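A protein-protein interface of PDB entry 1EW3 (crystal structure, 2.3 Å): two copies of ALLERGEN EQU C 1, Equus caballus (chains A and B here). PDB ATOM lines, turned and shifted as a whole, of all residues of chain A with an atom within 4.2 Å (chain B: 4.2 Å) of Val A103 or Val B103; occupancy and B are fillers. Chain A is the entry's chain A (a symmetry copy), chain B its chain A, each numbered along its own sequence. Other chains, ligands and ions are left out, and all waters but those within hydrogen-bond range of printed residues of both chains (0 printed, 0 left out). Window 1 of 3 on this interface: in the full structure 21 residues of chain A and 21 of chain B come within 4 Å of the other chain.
CG1 of Val A86 touches CZ of Phe B105, 3.4 Å away.
CG1 of Val B103 touches OH of Tyr A101, at 3.8 Å.
Val A103 touches Tyr B101.
Val A103 touches Val B103.
Val B86 touches Phe A105 (CG1 to CZ, 3.4 Å).
The backbone carbonyl oxygen (O) of Tyr B84 is in hydrogen-bond range of the backbone NH (N) of Phe B105 (3.0 Å).
The backbone carbonyl oxygen of Val B86 is in hydrogen-bond range of the backbone NH of Val B103, 2.9 Å away.
N of Phe A105 lies within hydrogen-bond range of O of Tyr A84.
The backbone carbonyl oxygen (O) of Val A86 sits at hydrogen-bond distance from the backbone NH (N) of Val A103 (2.9 Å).
Val A86 touches Phe B105, and with the chains exchanged Phe A105 touches Val B86.
Tyr A101 touches Val B103, and with the chains exchanged Val A103 touches Tyr B101.
Val A103 touches its own counterpart, Val B103.
Printed residues of chain B within 4 Å of Tyr A101: Val B103 (3.8 Å).
Printed residues of chain B within 4 Å of Val A103: Tyr B101 (3.8 Å) and Val B103 (3.95 Å).
Asn A104 touches none of the printed residues of chain B.
Printed residues of chain A within 4 Å of Tyr B101: Val A103.
Leu B102 touches none of the printed residues of chain A.
Of the printed residues of chain A, Phe B105 touches Val A86.
The nearest printed residue of chain B that does not touch Phe A105 is Tyr B101 (4.1 Å).
Printed residues of chain A that touch a printed residue of chain B: Val A86, Tyr A101, Val A103 and Phe A105.
Of the 9 printed residues of chain B, 4 touch a printed residue of chain A.
Printed residues of chain B that touch a printed residue of chain A: Val B86, Tyr B101, Val B103 and Phe B105.
Hydrophobic or aromatic side chains of chain B within 4 Å of the printed part of chain A: Val B86, Tyr B101, Val B103 and Phe B105.
Among the printed residues, 5 pairs touch across the chains.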
ATOM      1  N   TYR A  84     -17.921  30.469  12.302  1.00  0.00           N
ATOM      2  CA  TYR A  84     -16.558  30.695  11.812  1.00  0.00           C
ATOM      3  C   TYR A  84     -16.523  30.879  10.308  1.00  0.00           C
ATOM      4  O   TYR A  84     -17.067  30.039   9.591  1.00  0.00           O
ATOM      5  CB  TYR A  84     -15.733  29.505  12.260  1.00  0.00           C
ATOM      6  CG  TYR A  84     -14.265  29.670  11.952  1.00  0.00           C
ATOM      7  CD1 TYR A  84     -13.457  30.548  12.682  1.00  0.00           C
ATOM      8  CD2 TYR A  84     -13.732  28.931  10.904  1.00  0.00           C
ATOM      9  CE1 TYR A  84     -12.135  30.712  12.346  1.00  0.00           C
ATOM     10  CE2 TYR A  84     -12.394  29.057  10.612  1.00  0.00           C
ATOM     11  CZ  TYR A  84     -11.599  29.922  11.344  1.00  0.00           C
ATOM     12  OH  TYR A  84     -10.281  30.038  10.943  1.00  0.00           O
ATOM     13  N   ASN A  85     -15.873  31.891   9.801  1.00  0.00           N
ATOM     14  CA  ASN A  85     -15.838  32.258   8.417  1.00  0.00           C
ATOM     15  C   ASN A  85     -14.389  32.424   7.939  1.00  0.00           C
ATOM     16  O   ASN A  85     -13.604  32.963   8.701  1.00  0.00           O
ATOM     17  CB  ASN A  85     -16.498  33.686   8.244  1.00  0.00           C
ATOM     18  CG  ASN A  85     -17.908  33.688   8.823  1.00  0.00           C
ATOM     19  OD1 ASN A  85     -18.893  33.280   8.188  1.00  0.00           O
ATOM     20  ND2 ASN A  85     -18.063  34.070  10.093  1.00  0.00           N
ATOM     21  N   VAL A  86     -14.106  32.129   6.671  1.00  0.00           N
ATOM     22  CA  VAL A  86     -12.809  32.332   6.081  1.00  0.00           C
ATOM     23  C   VAL A  86     -13.101  33.002   4.768  1.00  0.00           C
ATOM     24  O   VAL A  86     -14.033  32.504   4.144  1.00  0.00           O
ATOM     25  CB  VAL A  86     -11.969  31.028   5.838  1.00  0.00           C
ATOM     26  CG1 VAL A  86     -10.783  31.395   4.961  1.00  0.00           C
ATOM     27  CG2 VAL A  86     -11.540  30.532   7.213  1.00  0.00           C
ATOM     28  N   TYR A 101     -14.829  36.855  -1.293  1.00  0.00           N
ATOM     29  CA  TYR A 101     -15.312  35.475  -1.340  1.00  0.00           C
ATOM     30  C   TYR A 101     -15.069  34.874   0.040  1.00  0.00           C
ATOM     31  O   TYR A 101     -13.937  34.757   0.509  1.00  0.00           O
ATOM     32  CB  TYR A 101     -14.467  34.703  -2.383  1.00  0.00           C
ATOM     33  CG  TYR A 101     -14.869  33.232  -2.383  1.00  0.00           C
ATOM     34  CD1 TYR A 101     -16.160  32.819  -2.698  1.00  0.00           C
ATOM     35  CD2 TYR A 101     -13.936  32.265  -2.062  1.00  0.00           C
ATOM     36  CE1 TYR A 101     -16.528  31.482  -2.638  1.00  0.00           C
ATOM     37  CE2 TYR A 101     -14.288  30.929  -2.037  1.00  0.00           C
ATOM     38  CZ  TYR A 101     -15.564  30.533  -2.333  1.00  0.00           C
ATOM     39  OH  TYR A 101     -15.871  29.205  -2.235  1.00  0.00           O
ATOM     40  N   LEU A 102     -16.121  34.474   0.714  1.00  0.00           N
ATOM     41  CA  LEU A 102     -16.284  33.976   2.021  1.00  0.00           C
ATOM     42  C   LEU A 102     -17.024  32.629   2.061  1.00  0.00           C
ATOM     43  O   LEU A 102     -17.997  32.443   1.361  1.00  0.00           O
ATOM     44  CB  LEU A 102     -17.022  35.032   2.855  1.00  0.00           C
ATOM     45  CG  LEU A 102     -17.390  34.677   4.280  1.00  0.00           C
ATOM     46  CD1 LEU A 102     -17.667  35.934   5.106  1.00  0.00           C
ATOM     47  CD2 LEU A 102     -18.600  33.750   4.302  1.00  0.00           C
ATOM     48  N   VAL A 103     -16.675  31.824   3.056  1.00  0.00           N
ATOM     49  CA  VAL A 103     -17.361  30.627   3.370  1.00  0.00           C
ATOM     50  C   VAL A 103     -17.539  30.618   4.877  1.00  0.00           C
ATOM     51  O   VAL A 103     -16.609  30.977   5.581  1.00  0.00           O
ATOM     52  CB  VAL A 103     -16.597  29.347   2.895  1.00  0.00           C
ATOM     53  CG1 VAL A 103     -17.245  28.086   3.371  1.00  0.00           C
ATOM     54  CG2 VAL A 103     -16.443  29.359   1.397  1.00  0.00           C
ATOM     55  N   ASN A 104     -18.684  30.178   5.330  1.00  0.00           N
ATOM     56  CA  ASN A 104     -19.035  30.001   6.717  1.00  0.00           C
ATOM     57  C   ASN A 104     -19.109  28.478   6.871  1.00  0.00           C
ATOM     58  O   ASN A 104     -19.884  27.770   6.216  1.00  0.00           O
ATOM     59  CB  ASN A 104     -20.439  30.672   6.888  1.00  0.00           C
ATOM     60  CG  ASN A 104     -20.903  30.563   8.318  1.00  0.00           C
ATOM     61  OD1 ASN A 104     -21.226  29.496   8.787  1.00  0.00           O
ATOM     62  ND2 ASN A 104     -20.912  31.667   9.063  1.00  0.00           N
ATOM     63  N   PHE A 105     -18.333  27.972   7.809  1.00  0.00           N
ATOM     64  CA  PHE A 105     -18.141  26.580   8.083  1.00  0.00           C
ATOM     65  C   PHE A 105     -19.112  26.058   9.108  1.00  0.00           C
ATOM     66  O   PHE A 105     -18.813  25.125   9.837  1.00  0.00           O
ATOM     67  CB  PHE A 105     -16.679  26.231   8.454  1.00  0.00           C
ATOM     68  CG  PHE A 105     -15.767  26.343   7.253  1.00  0.00           C
ATOM     69  CD1 PHE A 105     -15.197  27.535   6.885  1.00  0.00           C
ATOM     70  CD2 PHE A 105     -15.513  25.210   6.472  1.00  0.00           C
ATOM     71  CE1 PHE A 105     -14.384  27.636   5.759  1.00  0.00           C
ATOM     72  CE2 PHE A 105     -14.682  25.296   5.354  1.00  0.00           C
ATOM     73  CZ  PHE A 105     -14.133  26.486   4.973  1.00  0.00           C
ATOM     74  N   PHE A 111     -22.108  27.960   3.832  1.00  0.00           N
ATOM     75  CA  PHE A 111     -22.553  28.563   2.571  1.00  0.00           C
ATOM     76  C   PHE A 111     -21.409  29.419   2.075  1.00  0.00           C
ATOM     77  O   PHE A 111     -20.505  29.707   2.862  1.00  0.00           O
ATOM     78  CB  PHE A 111     -23.749  29.484   2.892  1.00  0.00           C
ATOM     79  CG  PHE A 111     -23.570  30.554   3.929  1.00  0.00           C
ATOM     80  CD1 PHE A 111     -23.066  31.800   3.618  1.00  0.00           C
ATOM     81  CD2 PHE A 111     -23.937  30.328   5.233  1.00  0.00           C
ATOM     82  CE1 PHE A 111     -22.981  32.809   4.570  1.00  0.00           C
ATOM     83  CE2 PHE A 111     -23.854  31.307   6.196  1.00  0.00           C
ATOM     84  CZ  PHE A 111     -23.378  32.561   5.850  1.00  0.00           C
ATOM     85  N   TYR B  84      -4.109  27.137  -0.216  1.00  0.00           N
ATOM     86  CA  TYR B  84      -4.612  27.144   1.160  1.00  0.00           C
ATOM     87  C   TYR B  84      -6.020  26.589   1.249  1.00  0.00           C
ATOM     88  O   TYR B  84      -6.889  27.047   0.508  1.00  0.00           O
ATOM     89  CB  TYR B  84      -4.533  28.578   1.645  1.00  0.00           C
ATOM     90  CG  TYR B  84      -4.882  28.714   3.106  1.00  0.00           C
ATOM     91  CD1 TYR B  84      -4.008  28.290   4.112  1.00  0.00           C
ATOM     92  CD2 TYR B  84      -6.115  29.264   3.433  1.00  0.00           C
ATOM     93  CE1 TYR B  84      -4.375  28.384   5.432  1.00  0.00           C
ATOM     94  CE2 TYR B  84      -6.451  29.409   4.759  1.00  0.00           C
ATOM     95  CZ  TYR B  84      -5.577  28.994   5.748  1.00  0.00           C
ATOM     96  OH  TYR B  84      -6.019  29.115   7.052  1.00  0.00           O
ATOM     97  N   ASN B  85      -6.295  25.678   2.141  1.00  0.00           N
ATOM     98  CA  ASN B  85      -7.541  24.984   2.277  1.00  0.00           C
ATOM     99  C   ASN B  85      -8.053  25.071   3.721  1.00  0.00           C
ATOM    100  O   ASN B  85      -7.232  24.966   4.616  1.00  0.00           O
ATOM    101  CB  ASN B  85      -7.305  23.441   2.013  1.00  0.00           C
ATOM    102  CG  ASN B  85      -6.655  23.235   0.649  1.00  0.00           C
ATOM    103  OD1 ASN B  85      -7.308  23.200  -0.405  1.00  0.00           O
ATOM    104  ND2 ASN B  85      -5.322  23.170   0.594  1.00  0.00           N
ATOM    105  N   VAL B  86      -9.370  25.087   3.922  1.00  0.00           N
ATOM    106  CA  VAL B  86      -9.971  25.072   5.231  1.00  0.00           C
ATOM    107  C   VAL B  86     -11.051  24.031   5.128  1.00  0.00           C
ATOM    108  O   VAL B  86     -11.719  24.097   4.101  1.00  0.00           O
ATOM    109  CB  VAL B  86     -10.590  26.436   5.702  1.00  0.00           C
ATOM    110  CG1 VAL B  86     -11.419  26.165   6.947  1.00  0.00           C
ATOM    111  CG2 VAL B  86      -9.415  27.365   5.981  1.00  0.00           C
ATOM    112  N   TYR B 101     -15.818  18.424   4.490  1.00  0.00           N
ATOM    113  CA  TYR B 101     -16.181  19.576   3.664  1.00  0.00           C
ATOM    114  C   TYR B 101     -15.016  20.557   3.737  1.00  0.00           C
ATOM    115  O   TYR B 101     -14.665  21.074   4.796  1.00  0.00           O
ATOM    116  CB  TYR B 101     -17.438  20.237   4.283  1.00  0.00           C
ATOM    117  CG  TYR B 101     -17.783  21.506   3.511  1.00  0.00           C
ATOM    118  CD1 TYR B 101     -18.109  21.483   2.158  1.00  0.00           C
ATOM    119  CD2 TYR B 101     -17.777  22.727   4.159  1.00  0.00           C
ATOM    120  CE1 TYR B 101     -18.366  22.651   1.455  1.00  0.00           C
ATOM    121  CE2 TYR B 101     -18.068  23.889   3.471  1.00  0.00           C
ATOM    122  CZ  TYR B 101     -18.373  23.859   2.137  1.00  0.00           C
ATOM    123  OH  TYR B 101     -18.594  25.044   1.494  1.00  0.00           O
ATOM    124  N   LEU B 102     -14.399  20.840   2.614  1.00  0.00           N
ATOM    125  CA  LEU B 102     -13.253  21.603   2.321  1.00  0.00           C
ATOM    126  C   LEU B 102     -13.507  22.682   1.255  1.00  0.00           C
ATOM    127  O   LEU B 102     -14.168  22.426   0.271  1.00  0.00           O
ATOM    128  CB  LEU B 102     -12.133  20.650   1.881  1.00  0.00           C
ATOM    129  CG  LEU B 102     -10.824  21.259   1.427  1.00  0.00           C
ATOM    130  CD1 LEU B 102      -9.691  20.234   1.483  1.00  0.00           C
ATOM    131  CD2 LEU B 102     -10.959  21.823   0.016  1.00  0.00           C
ATOM    132  N   VAL B 103     -12.773  23.779   1.379  1.00  0.00           N
ATOM    133  CA  VAL B 103     -12.728  24.804   0.403  1.00  0.00           C
ATOM    134  C   VAL B 103     -11.264  25.159   0.222  1.00  0.00           C
ATOM    135  O   VAL B 103     -10.553  25.243   1.211  1.00  0.00           O
ATOM    136  CB  VAL B 103     -13.559  26.065   0.808  1.00  0.00           C
ATOM    137  CG1 VAL B 103     -13.377  27.201  -0.148  1.00  0.00           C
ATOM    138  CG2 VAL B 103     -15.012  25.702   0.966  1.00  0.00           C
ATOM    139  N   ASN B 104     -10.865  25.398  -1.000  1.00  0.00           N
ATOM    140  CA  ASN B 104      -9.548  25.836  -1.391  1.00  0.00           C
ATOM    141  C   ASN B 104      -9.779  27.277  -1.860  1.00  0.00           C
ATOM    142  O   ASN B 104     -10.541  27.570  -2.790  1.00  0.00           O
ATOM    143  CB  ASN B 104      -9.123  24.900  -2.571  1.00  0.00           C
ATOM    144  CG  ASN B 104      -7.740  25.257  -3.054  1.00  0.00           C
ATOM    145  OD1 ASN B 104      -7.537  26.293  -3.646  1.00  0.00           O
ATOM    146  ND2 ASN B 104      -6.742  24.421  -2.778  1.00  0.00           N
ATOM    147  N   PHE B 105      -9.051  28.189  -1.246  1.00  0.00           N
ATOM    148  CA  PHE B 105      -9.150  29.605  -1.425  1.00  0.00           C
ATOM    149  C   PHE B 105      -8.231  30.113  -2.503  1.00  0.00           C
ATOM    150  O   PHE B 105      -7.782  31.249  -2.461  1.00  0.00           O
ATOM    151  CB  PHE B 105      -8.974  30.397  -0.106  1.00  0.00           C
ATOM    152  CG  PHE B 105     -10.164  30.210   0.809  1.00  0.00           C
ATOM    153  CD1 PHE B 105     -10.254  29.148   1.671  1.00  0.00           C
ATOM    154  CD2 PHE B 105     -11.221  31.126   0.762  1.00  0.00           C
ATOM    155  CE1 PHE B 105     -11.368  28.965   2.487  1.00  0.00           C
ATOM    156  CE2 PHE B 105     -12.331  30.965   1.591  1.00  0.00           C
ATOM    157  CZ  PHE B 105     -12.434  29.896   2.433  1.00  0.00           C
ATOM    158  N   PHE B 111     -12.651  26.209  -4.877  1.00  0.00           N
ATOM    159  CA  PHE B 111     -13.689  25.207  -5.145  1.00  0.00           C
ATOM    160  C   PHE B 111     -14.024  24.569  -3.815  1.00  0.00           C
ATOM    161  O   PHE B 111     -13.250  24.734  -2.870  1.00  0.00           O
ATOM    162  CB  PHE B 111     -13.069  24.130  -6.061  1.00  0.00           C
ATOM    163  CG  PHE B 111     -11.809  23.448  -5.613  1.00  0.00           C
ATOM    164  CD1 PHE B 111     -11.827  22.333  -4.801  1.00  0.00           C
ATOM    165  CD2 PHE B 111     -10.584  23.905  -6.031  1.00  0.00           C
ATOM    166  CE1 PHE B 111     -10.658  21.663  -4.459  1.00  0.00           C
ATOM    167  CE2 PHE B 111      -9.412  23.266  -5.700  1.00  0.00           C
ATOM    168  CZ  PHE B 111      -9.460  22.128  -4.912  1.00  0.00           C
